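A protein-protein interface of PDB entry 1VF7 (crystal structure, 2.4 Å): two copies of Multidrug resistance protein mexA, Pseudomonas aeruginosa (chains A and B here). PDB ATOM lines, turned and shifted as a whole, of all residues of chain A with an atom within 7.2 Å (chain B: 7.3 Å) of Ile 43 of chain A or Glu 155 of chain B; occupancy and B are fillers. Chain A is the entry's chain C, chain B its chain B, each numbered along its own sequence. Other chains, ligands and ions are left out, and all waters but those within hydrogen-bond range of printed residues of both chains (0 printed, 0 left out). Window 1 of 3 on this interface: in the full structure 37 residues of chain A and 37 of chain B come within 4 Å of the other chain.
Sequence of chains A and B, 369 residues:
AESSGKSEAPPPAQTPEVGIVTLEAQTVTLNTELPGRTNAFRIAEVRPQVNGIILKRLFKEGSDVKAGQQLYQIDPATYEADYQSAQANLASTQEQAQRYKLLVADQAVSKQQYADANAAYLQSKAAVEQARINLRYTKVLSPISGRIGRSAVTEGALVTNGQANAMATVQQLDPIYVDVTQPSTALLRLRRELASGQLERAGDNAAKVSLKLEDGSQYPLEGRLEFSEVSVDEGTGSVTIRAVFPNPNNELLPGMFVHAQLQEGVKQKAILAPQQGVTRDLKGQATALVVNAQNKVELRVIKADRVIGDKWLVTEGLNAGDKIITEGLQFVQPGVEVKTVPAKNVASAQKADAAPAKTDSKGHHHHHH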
ATOM      1  N   ASN A  39     -16.706  20.940  -0.317  1.00  0.00           N
ATOM      2  CA  ASN A  39     -16.868  21.900   0.747  1.00  0.00           C
ATOM      3  C   ASN A  39     -15.727  21.697   1.738  1.00  0.00           C
ATOM      4  O   ASN A  39     -15.240  20.553   1.917  1.00  0.00           O
ATOM      5  CB  ASN A  39     -18.163  21.650   1.497  1.00  0.00           C
ATOM      6  CG  ASN A  39     -19.354  22.185   0.764  1.00  0.00           C
ATOM      7  OD1 ASN A  39     -19.330  23.311   0.259  1.00  0.00           O
ATOM      8  ND2 ASN A  39     -20.424  21.375   0.678  1.00  0.00           N
ATOM      9  N   ALA A  40     -15.320  22.784   2.406  1.00  0.00           N
ATOM     10  CA  ALA A  40     -14.301  22.671   3.430  1.00  0.00           C
ATOM     11  C   ALA A  40     -14.749  21.753   4.573  1.00  0.00           C
ATOM     12  O   ALA A  40     -15.926  21.646   4.933  1.00  0.00           O
ATOM     13  CB  ALA A  40     -13.823  24.084   3.953  1.00  0.00           C
ATOM     14  N   PHE A  41     -13.779  21.057   5.115  1.00  0.00           N
ATOM     15  CA  PHE A  41     -14.000  20.196   6.252  1.00  0.00           C
ATOM     16  C   PHE A  41     -14.311  21.060   7.488  1.00  0.00           C
ATOM     17  O   PHE A  41     -15.210  20.743   8.265  1.00  0.00           O
ATOM     18  CB  PHE A  41     -12.751  19.331   6.426  1.00  0.00           C
ATOM     19  CG  PHE A  41     -12.950  18.139   7.323  1.00  0.00           C
ATOM     20  CD1 PHE A  41     -13.766  17.080   6.927  1.00  0.00           C
ATOM     21  CD2 PHE A  41     -12.305  18.062   8.553  1.00  0.00           C
ATOM     22  CE1 PHE A  41     -13.964  15.989   7.765  1.00  0.00           C
ATOM     23  CE2 PHE A  41     -12.467  16.954   9.379  1.00  0.00           C
ATOM     24  CZ  PHE A  41     -13.308  15.910   8.974  1.00  0.00           C
ATOM     25  N   ARG A  42     -13.579  22.179   7.631  1.00  0.00           N
ATOM     26  CA  ARG A  42     -13.738  23.132   8.733  1.00  0.00           C
ATOM     27  C   ARG A  42     -13.356  24.527   8.231  1.00  0.00           C
ATOM     28  O   ARG A  42     -12.408  24.703   7.452  1.00  0.00           O
ATOM     29  CB  ARG A  42     -12.850  22.746   9.942  1.00  0.00           C
ATOM     30  CG  ARG A  42     -13.619  22.728  11.255  1.00  0.00           C
ATOM     31  CD  ARG A  42     -12.835  22.231  12.481  1.00  0.00           C
ATOM     32  NE  ARG A  42     -13.697  21.512  13.472  1.00  0.00           N
ATOM     33  CZ  ARG A  42     -14.702  22.057  14.169  1.00  0.00           C
ATOM     34  NH1 ARG A  42     -15.001  23.332  14.004  1.00  0.00           N
ATOM     35  NH2 ARG A  42     -15.392  21.347  15.047  1.00  0.00           N
ATOM     36  N   ILE A  43     -14.108  25.506   8.692  1.00  0.00           N
ATOM     37  CA  ILE A  43     -13.907  26.902   8.390  1.00  0.00           C
ATOM     38  C   ILE A  43     -13.811  27.648   9.720  1.00  0.00           C
ATOM     39  O   ILE A  43     -14.555  27.349  10.674  1.00  0.00           O
ATOM     40  CB  ILE A  43     -15.088  27.421   7.514  1.00  0.00           C
ATOM     41  CG1 ILE A  43     -15.215  26.541   6.253  1.00  0.00           C
ATOM     42  CG2 ILE A  43     -14.894  28.904   7.141  1.00  0.00           C
ATOM     43  CD1 ILE A  43     -16.278  27.027   5.157  1.00  0.00           C
ATOM     44  N   ALA A  44     -12.855  28.576   9.806  1.00  0.00           N
ATOM     45  CA  ALA A  44     -12.738  29.507  10.951  1.00  0.00           C
ATOM     46  C   ALA A  44     -12.498  30.923  10.418  1.00  0.00           C
ATOM     47  O   ALA A  44     -11.798  31.076   9.445  1.00  0.00           O
ATOM     48  CB  ALA A  44     -11.648  29.109  11.846  1.00  0.00           C
ATOM     49  N   GLU A  45     -13.125  31.926  11.020  1.00  0.00           N
ATOM     50  CA  GLU A  45     -12.846  33.345  10.749  1.00  0.00           C
ATOM     51  C   GLU A  45     -11.794  33.912  11.753  1.00  0.00           C
ATOM     52  O   GLU A  45     -11.684  33.434  12.850  1.00  0.00           O
ATOM     53  CB  GLU A  45     -14.128  34.144  10.928  1.00  0.00           C
ATOM     54  CG  GLU A  45     -15.169  33.899   9.878  1.00  0.00           C
ATOM     55  CD  GLU A  45     -16.439  34.681  10.163  1.00  0.00           C
ATOM     56  OE1 GLU A  45     -16.424  35.614  11.001  1.00  0.00           O
ATOM     57  OE2 GLU A  45     -17.476  34.381   9.570  1.00  0.00           O
ATOM     58  N   VAL A  46     -11.030  34.902  11.328  1.00  0.00           N
ATOM     59  CA  VAL A  46     -10.021  35.562  12.134  1.00  0.00           C
ATOM     60  C   VAL A  46     -10.502  37.007  12.326  1.00  0.00           C
ATOM     61  O   VAL A  46     -10.800  37.723  11.350  1.00  0.00           O
ATOM     62  CB  VAL A  46      -8.672  35.559  11.390  1.00  0.00           C
ATOM     63  CG1 VAL A  46      -7.513  36.162  12.228  1.00  0.00           C
ATOM     64  CG2 VAL A  46      -8.261  34.098  10.934  1.00  0.00           C
ATOM     65  N   ARG A  47     -10.650  37.412  13.586  1.00  0.00           N
ATOM     66  CA  ARG A  47     -11.275  38.657  13.933  1.00  0.00           C
ATOM     67  C   ARG A  47     -10.476  39.274  15.085  1.00  0.00           C
ATOM     68  O   ARG A  47      -9.884  38.562  15.917  1.00  0.00           O
ATOM     69  CB  ARG A  47     -12.742  38.422  14.384  1.00  0.00           C
ATOM     70  CG  ARG A  47     -13.664  37.997  13.277  1.00  0.00           C
ATOM     71  CD  ARG A  47     -15.091  37.822  13.724  1.00  0.00           C
ATOM     72  NE  ARG A  47     -15.959  37.763  12.560  1.00  0.00           N
ATOM     73  CZ  ARG A  47     -16.623  38.772  12.005  1.00  0.00           C
ATOM     74  NH1 ARG A  47     -16.580  39.994  12.512  1.00  0.00           N
ATOM     75  NH2 ARG A  47     -17.355  38.547  10.894  1.00  0.00           N
ATOM     76  N   PRO A 143      -7.512  30.413  14.565  1.00  0.00           N
ATOM     77  CA  PRO A 143      -8.301  29.506  15.405  1.00  0.00           C
ATOM     78  C   PRO A 143      -8.068  28.008  15.027  1.00  0.00           C
ATOM     79  O   PRO A 143      -8.186  27.142  15.902  1.00  0.00           O
ATOM     80  CB  PRO A 143      -9.740  29.924  15.113  1.00  0.00           C
ATOM     81  CG  PRO A 143      -9.613  31.316  14.545  1.00  0.00           C
ATOM     82  CD  PRO A 143      -8.366  31.190  13.636  1.00  0.00           C
ATOM     83  N   ILE A 144      -7.744  27.680  13.775  1.00  0.00           N
ATOM     84  CA  ILE A 144      -7.573  26.265  13.376  1.00  0.00           C
ATOM     85  C   ILE A 144      -6.398  26.105  12.404  1.00  0.00           C
ATOM     86  O   ILE A 144      -5.887  27.109  11.845  1.00  0.00           O
ATOM     87  CB  ILE A 144      -8.882  25.702  12.687  1.00  0.00           C
ATOM     88  CG1 ILE A 144      -9.126  26.417  11.345  1.00  0.00           C
ATOM     89  CG2 ILE A 144     -10.113  25.851  13.628  1.00  0.00           C
ATOM     90  CD1 ILE A 144     -10.209  25.861  10.409  1.00  0.00           C
ATOM     91  N   THR A 169      -9.869  34.115   6.659  1.00  0.00           N
ATOM     92  CA  THR A 169     -10.656  32.875   6.776  1.00  0.00           C
ATOM     93  C   THR A 169      -9.697  31.700   6.586  1.00  0.00           C
ATOM     94  O   THR A 169      -8.946  31.645   5.626  1.00  0.00           O
ATOM     95  CB  THR A 169     -11.773  32.842   5.715  1.00  0.00           C
ATOM     96  OG1 THR A 169     -12.710  33.893   5.973  1.00  0.00           O
ATOM     97  CG2 THR A 169     -12.698  31.581   5.893  1.00  0.00           C
ATOM     98  N   VAL A 170      -9.704  30.744   7.510  1.00  0.00           N
ATOM     99  CA  VAL A 170      -8.921  29.540   7.349  1.00  0.00           C
ATOM    100  C   VAL A 170      -9.908  28.390   7.070  1.00  0.00           C
ATOM    101  O   VAL A 170     -10.941  28.261   7.730  1.00  0.00           O
ATOM    102  CB  VAL A 170      -8.086  29.284   8.598  1.00  0.00           C
ATOM    103  CG1 VAL A 170      -7.099  28.089   8.436  1.00  0.00           C
ATOM    104  CG2 VAL A 170      -7.274  30.574   8.954  1.00  0.00           C
ATOM    105  N   GLN A 171      -9.586  27.569   6.068  1.00  0.00           N
ATOM    106  CA  GLN A 171     -10.398  26.384   5.680  1.00  0.00           C
ATOM    107  C   GLN A 171      -9.565  25.155   5.699  1.00  0.00           C
ATOM    108  O   GLN A 171      -8.524  25.100   5.087  1.00  0.00           O
ATOM    109  CB  GLN A 171     -10.946  26.580   4.304  1.00  0.00           C
ATOM    110  CG  GLN A 171     -11.850  27.742   4.282  1.00  0.00           C
ATOM    111  CD  GLN A 171     -12.521  27.931   2.991  1.00  0.00           C
ATOM    112  OE1 GLN A 171     -13.155  27.028   2.487  1.00  0.00           O
ATOM    113  NE2 GLN A 171     -12.437  29.121   2.456  1.00  0.00           N
ATOM    114  N   GLN A 172      -9.950  24.203   6.503  1.00  0.00           N
ATOM    115  CA  GLN A 172      -9.291  22.897   6.455  1.00  0.00           C
ATOM    116  C   GLN A 172      -9.792  22.132   5.205  1.00  0.00           C
ATOM    117  O   GLN A 172     -11.003  21.954   4.980  1.00  0.00           O
ATOM    118  CB  GLN A 172      -9.480  22.097   7.740  1.00  0.00           C
ATOM    119  CG  GLN A 172      -8.801  20.780   7.643  1.00  0.00           C
ATOM    120  CD  GLN A 172      -9.112  19.878   8.813  1.00  0.00           C
ATOM    121  OE1 GLN A 172      -9.804  20.308   9.746  1.00  0.00           O
ATOM    122  NE2 GLN A 172      -8.601  18.622   8.780  1.00  0.00           N
ATOM    123  N   PRO A 254     -13.150  23.656  -2.545  1.00  0.00           N
ATOM    124  CA  PRO A 254     -14.572  23.795  -2.359  1.00  0.00           C
ATOM    125  C   PRO A 254     -15.211  24.271  -3.649  1.00  0.00           C
ATOM    126  O   PRO A 254     -14.504  24.786  -4.521  1.00  0.00           O
ATOM    127  CB  PRO A 254     -14.662  24.841  -1.250  1.00  0.00           C
ATOM    128  CG  PRO A 254     -13.429  24.588  -0.472  1.00  0.00           C
ATOM    129  CD  PRO A 254     -12.372  24.324  -1.481  1.00  0.00           C
ATOM    130  N   ILE B  53     -16.886  36.337  20.581  1.00  0.00           N
ATOM    131  CA  ILE B  53     -16.277  35.486  19.585  1.00  0.00           C
ATOM    132  C   ILE B  53     -16.439  34.002  19.942  1.00  0.00           C
ATOM    133  O   ILE B  53     -16.181  33.575  21.122  1.00  0.00           O
ATOM    134  CB  ILE B  53     -14.757  35.841  19.519  1.00  0.00           C
ATOM    135  CG1 ILE B  53     -14.603  37.280  18.960  1.00  0.00           C
ATOM    136  CG2 ILE B  53     -13.932  34.733  18.697  1.00  0.00           C
ATOM    137  CD1 ILE B  53     -14.807  37.419  17.431  1.00  0.00           C
ATOM    138  N   ILE B  54     -16.844  33.234  18.932  1.00  0.00           N
ATOM    139  CA  ILE B  54     -16.851  31.776  19.053  1.00  0.00           C
ATOM    140  C   ILE B  54     -15.419  31.221  19.121  1.00  0.00           C
ATOM    141  O   ILE B  54     -14.716  31.179  18.094  1.00  0.00           O
ATOM    142  CB  ILE B  54     -17.606  31.057  17.879  1.00  0.00           C
ATOM    143  CG1 ILE B  54     -19.051  31.535  17.713  1.00  0.00           C
ATOM    144  CG2 ILE B  54     -17.600  29.498  18.132  1.00  0.00           C
ATOM    145  CD1 ILE B  54     -19.806  31.317  18.977  1.00  0.00           C
ATOM    146  N   LEU B  55     -15.047  30.702  20.287  1.00  0.00           N
ATOM    147  CA  LEU B  55     -13.837  29.914  20.429  1.00  0.00           C
ATOM    148  C   LEU B  55     -13.963  28.453  19.922  1.00  0.00           C
ATOM    149  O   LEU B  55     -13.019  27.909  19.339  1.00  0.00           O
ATOM    150  CB  LEU B  55     -13.372  29.863  21.895  1.00  0.00           C
ATOM    151  CG  LEU B  55     -12.528  30.937  22.557  1.00  0.00           C
ATOM    152  CD1 LEU B  55     -11.918  30.437  23.936  1.00  0.00           C
ATOM    153  CD2 LEU B  55     -11.431  31.509  21.611  1.00  0.00           C
ATOM    154  N   LYS B  56     -15.076  27.783  20.204  1.00  0.00           N
ATOM    155  CA  LYS B  56     -15.213  26.372  19.823  1.00  0.00           C
ATOM    156  C   LYS B  56     -16.639  26.042  19.490  1.00  0.00           C
ATOM    157  O   LYS B  56     -17.575  26.468  20.197  1.00  0.00           O
ATOM    158  CB  LYS B  56     -14.808  25.445  20.956  1.00  0.00           C
ATOM    159  CG  LYS B  56     -13.406  25.585  21.445  1.00  0.00           C
ATOM    160  CD  LYS B  56     -12.460  24.799  20.525  1.00  0.00           C
ATOM    161  CE  LYS B  56     -10.959  25.363  20.599  1.00  0.00           C
ATOM    162  NZ  LYS B  56     -10.117  24.673  19.526  1.00  0.00           N
ATOM    163  N   ARG B  57     -16.789  25.296  18.405  1.00  0.00           N
ATOM    164  CA  ARG B  57     -18.011  24.644  18.110  1.00  0.00           C
ATOM    165  C   ARG B  57     -18.226  23.355  18.881  1.00  0.00           C
ATOM    166  O   ARG B  57     -19.323  23.175  19.453  1.00  0.00           O
ATOM    167  CB  ARG B  57     -18.210  24.413  16.662  1.00  0.00           C
ATOM    168  CG  ARG B  57     -19.443  23.589  16.304  1.00  0.00           C
ATOM    169  CD  ARG B  57     -19.511  23.493  14.786  1.00  0.00           C
ATOM    170  NE  ARG B  57     -19.139  22.168  14.511  1.00  0.00           N
ATOM    171  CZ  ARG B  57     -18.458  21.722  13.519  1.00  0.00           C
ATOM    172  NH1 ARG B  57     -17.987  22.485  12.551  1.00  0.00           N
ATOM    173  NH2 ARG B  57     -18.231  20.421  13.546  1.00  0.00           N
ATOM    174  N   LEU B  58     -17.323  22.424  19.045  1.00  0.00           N
ATOM    175  CA  LEU B  58     -17.895  21.405  20.104  1.00  0.00           C
ATOM    176  C   LEU B  58     -18.952  20.327  19.791  1.00  0.00           C
ATOM    177  O   LEU B  58     -19.099  19.431  20.595  1.00  0.00           O
ATOM    178  CB  LEU B  58     -18.372  21.991  21.448  1.00  0.00           C
ATOM    179  CG  LEU B  58     -17.369  22.854  22.262  1.00  0.00           C
ATOM    180  CD1 LEU B  58     -17.982  23.372  23.520  1.00  0.00           C
ATOM    181  CD2 LEU B  58     -16.022  22.114  22.558  1.00  0.00           C
ATOM    182  N   PHE B  59     -19.678  20.364  18.687  1.00  0.00           N
ATOM    183  CA  PHE B  59     -20.482  19.208  18.305  1.00  0.00           C
ATOM    184  C   PHE B  59     -20.190  18.915  16.891  1.00  0.00           C
ATOM    185  O   PHE B  59     -19.709  19.763  16.156  1.00  0.00           O
ATOM    186  CB  PHE B  59     -21.983  19.436  18.442  1.00  0.00           C
ATOM    187  CG  PHE B  59     -22.490  20.618  17.616  1.00  0.00           C
ATOM    188  CD1 PHE B  59     -22.892  20.437  16.306  1.00  0.00           C
ATOM    189  CD2 PHE B  59     -22.501  21.924  18.163  1.00  0.00           C
ATOM    190  CE1 PHE B  59     -23.335  21.508  15.516  1.00  0.00           C
ATOM    191  CE2 PHE B  59     -22.950  23.014  17.393  1.00  0.00           C
ATOM    192  CZ  PHE B  59     -23.356  22.824  16.064  1.00  0.00           C
ATOM    193  N   TYR B  72     -21.427  25.354  22.109  1.00  0.00           N
ATOM    194  CA  TYR B  72     -20.427  26.338  21.730  1.00  0.00           C
ATOM    195  C   TYR B  72     -19.721  26.940  22.945  1.00  0.00           C
ATOM    196  O   TYR B  72     -20.290  27.119  24.016  1.00  0.00           O
ATOM    197  CB  TYR B  72     -21.049  27.478  20.960  1.00  0.00           C
ATOM    198  CG  TYR B  72     -21.669  27.144  19.616  1.00  0.00           C
ATOM    199  CD1 TYR B  72     -23.052  26.794  19.529  1.00  0.00           C
ATOM    200  CD2 TYR B  72     -20.927  27.215  18.428  1.00  0.00           C
ATOM    201  CE1 TYR B  72     -23.662  26.537  18.302  1.00  0.00           C
ATOM    202  CE2 TYR B  72     -21.565  26.902  17.173  1.00  0.00           C
ATOM    203  CZ  TYR B  72     -22.923  26.567  17.154  1.00  0.00           C
ATOM    204  OH  TYR B  72     -23.595  26.303  15.963  1.00  0.00           O
ATOM    205  N   GLN B  73     -18.460  27.269  22.764  1.00  0.00           N
ATOM    206  CA  GLN B  73     -17.793  28.139  23.761  1.00  0.00           C
ATOM    207  C   GLN B  73     -17.580  29.548  23.147  1.00  0.00           C
ATOM    208  O   GLN B  73     -16.910  29.698  22.120  1.00  0.00           O
ATOM    209  CB  GLN B  73     -16.455  27.523  24.185  1.00  0.00           C
ATOM    210  CG  GLN B  73     -15.704  28.386  25.210  1.00  0.00           C
ATOM    211  CD  GLN B  73     -16.347  28.420  26.576  1.00  0.00           C
ATOM    212  OE1 GLN B  73     -16.527  27.382  27.232  1.00  0.00           O
ATOM    213  NE2 GLN B  73     -16.662  29.586  27.027  1.00  0.00           N
ATOM    214  N   SER B 151     -23.933  23.819  11.751  1.00  0.00           N
ATOM    215  CA  SER B 151     -23.707  25.090  12.422  1.00  0.00           C
ATOM    216  C   SER B 151     -23.833  26.222  11.403  1.00  0.00           C
ATOM    217  O   SER B 151     -23.130  26.202  10.413  1.00  0.00           O
ATOM    218  CB  SER B 151     -22.282  25.064  12.981  1.00  0.00           C
ATOM    219  OG  SER B 151     -22.175  26.087  13.948  1.00  0.00           O
ATOM    220  N   VAL B 153     -22.805  29.105  12.035  1.00  0.00           N
ATOM    221  CA  VAL B 153     -21.777  30.039  12.488  1.00  0.00           C
ATOM    222  C   VAL B 153     -20.467  29.272  12.607  1.00  0.00           C
ATOM    223  O   VAL B 153     -20.450  28.182  13.169  1.00  0.00           O
ATOM    224  CB  VAL B 153     -22.219  30.642  13.882  1.00  0.00           C
ATOM    225  CG1 VAL B 153     -21.128  31.254  14.519  1.00  0.00           C
ATOM    226  CG2 VAL B 153     -23.319  31.722  13.673  1.00  0.00           C
ATOM    227  N   THR B 154     -19.369  29.802  12.087  1.00  0.00           N
ATOM    228  CA  THR B 154     -18.080  29.118  12.307  1.00  0.00           C
ATOM    229  C   THR B 154     -17.365  29.509  13.561  1.00  0.00           C
ATOM    230  O   THR B 154     -17.683  30.480  14.214  1.00  0.00           O
ATOM    231  CB  THR B 154     -17.131  29.318  11.168  1.00  0.00           C
ATOM    232  OG1 THR B 154     -16.866  30.722  11.043  1.00  0.00           O
ATOM    233  CG2 THR B 154     -17.819  28.917   9.845  1.00  0.00           C
ATOM    234  N   GLU B 155     -16.394  28.717  13.915  1.00  0.00           N
ATOM    235  CA  GLU B 155     -15.437  29.135  14.911  1.00  0.00           C
ATOM    236  C   GLU B 155     -14.795  30.450  14.458  1.00  0.00           C
ATOM    237  O   GLU B 155     -14.669  30.706  13.247  1.00  0.00           O
ATOM    238  CB  GLU B 155     -14.409  28.052  15.160  1.00  0.00           C
ATOM    239  CG  GLU B 155     -15.029  26.938  16.018  1.00  0.00           C
ATOM    240  CD  GLU B 155     -14.115  25.738  16.263  1.00  0.00           C
ATOM    241  OE1 GLU B 155     -14.481  24.825  17.063  1.00  0.00           O
ATOM    242  OE2 GLU B 155     -13.002  25.718  15.676  1.00  0.00           O
ATOM    243  N   GLY B 156     -14.446  31.277  15.443  1.00  0.00           N
ATOM    244  CA  GLY B 156     -13.892  32.562  15.199  1.00  0.00           C
ATOM    245  C   GLY B 156     -14.927  33.562  14.804  1.00  0.00           C
ATOM    246  O   GLY B 156     -14.615  34.722  14.641  1.00  0.00           O
ATOM    247  N   ALA B 157     -16.174  33.138  14.610  1.00  0.00           N
ATOM    248  CA  ALA B 157     -17.173  34.116  14.224  1.00  0.00           C
ATOM    249  C   ALA B 157     -17.564  34.965  15.410  1.00  0.00           C
ATOM    250  O   ALA B 157     -17.490  34.535  16.575  1.00  0.00           O
ATOM    251  CB  ALA B 157     -18.416  33.449  13.664  1.00  0.00           C
ATOM    252  N   LEU B 158     -18.105  36.127  15.073  1.00  0.00           N
ATOM    253  CA  LEU B 158     -18.704  37.039  16.007  1.00  0.00           C
ATOM    254  C   LEU B 158     -20.196  36.784  16.195  1.00  0.00           C
ATOM    255  O   LEU B 158     -20.926  36.768  15.220  1.00  0.00           O
ATOM    256  CB  LEU B 158     -18.516  38.452  15.418  1.00  0.00           C
ATOM    257  CG  LEU B 158     -19.046  39.616  16.228  1.00  0.00           C
ATOM    258  CD1 LEU B 158     -18.141  39.891  17.437  1.00  0.00           C
ATOM    259  CD2 LEU B 158     -19.287  40.854  15.370  1.00  0.00           C
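OE1 of Glu 155 of chain B is in salt-bridge range of NH1 of Arg 42 of chain A. The backbone carbonyl oxygen of Glu 155 of chain B sits at hydrogen-bond distance from the backbone NH of Glu 45 of chain A. The guanidinium group (NH2) of Arg 42 of chain A lies close to the guanidinium group (NH2) of Arg 57 of chain B, 3.3 Å away.
Ile 43 of chain A touches just these residues of chain B: Thr 154 and Glu 155. Glu 155 of chain B touches just these residues of chain A: Arg 42 (3.4 Å), Ile 43 (3.97 Å), Ala 44 (3.2 Å), Glu 45 (3.0 Å) and Ile 144 (3.5 Å). Of the printed residues of chain B, Arg 47 of chain A touches Ile 53, Gly 156 and Leu 158. Of the printed residues of chain B, Glu 45 of chain A touches Thr 154, Glu 155, Gly 156 and Ala 157. Of the printed residues of chain A, Thr 154 of chain B touches Ile 43 and Glu 45. The nearest residue of chain B that does not touch Ile 43 of chain A is Gly 156 of chain B (6.2 Å). The nearest residue of chain A that does not touch Glu 155 of chain B is Pro 143 of chain A (5.0 Å).
No position is printed for both chains.
Printed residues of chain B that touch a printed residue of chain A: Ile 53, Arg 57, Thr 154, Glu 155, Gly 156, Ala 157 and Leu 158. Hydrophobic or aromatic side chains of chain B that line the printed part of chain A: Ile 53, Ala 157 and Leu 158. Among the printed residues, 13 pairs touch across the chains. Among the printed residues, Asp or Glu carboxylates within 4 Å of a Lys or Arg side-chain nitrogen of the other chain: Arg 42 of chain A with Glu 155 of chain B (3.4 Å).
O of Ile 54 of chain B sits at hydrogen-bond distance from N of Gly 156 of chain B, 2.7 Å away. O of Ala 157 of chain B lies within hydrogen-bond range of N of Ile 54 of chain B. NE of Arg 57 of chain B lies within hydrogen-bond range of O of Phe 59 of chain B, at 3.0 Å. N of Arg 57 of chain B lies within hydrogen-bond range of OE1 of Glu 155 of chain B. The backbone carbonyl oxygen (O) of Arg 42 of chain A sits at hydrogen-bond distance from the backbone NH (N) of Gln 172 of chain A (2.7 Å). The backbone carbonyl oxygen (O) of Val 170 of chain A sits at hydrogen-bond distance from the backbone NH (N) of Ala 44 of chain A (2.8 Å).
Among the printed residues, merely in contact across the chains: Ile 43 of chain A with Thr 154 of chain B, Ile 43 of chain A with Glu 155 of chain B, Ala 44 of chain A with Glu 155 of chain B, Glu 45 of chain A with Thr 154 of chain B, Glu 45 of chain A with Gly 156 of chain B, Glu 45 of chain A with Ala 157 of chain B, Arg 47 of chain A with Ile 53 of chain B, Arg 47 of chain A with Gly 156 of chain B, Arg 47 of chain A with Leu 158 of chain B and Ile 144 of chain A with Glu 155 of chain B.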
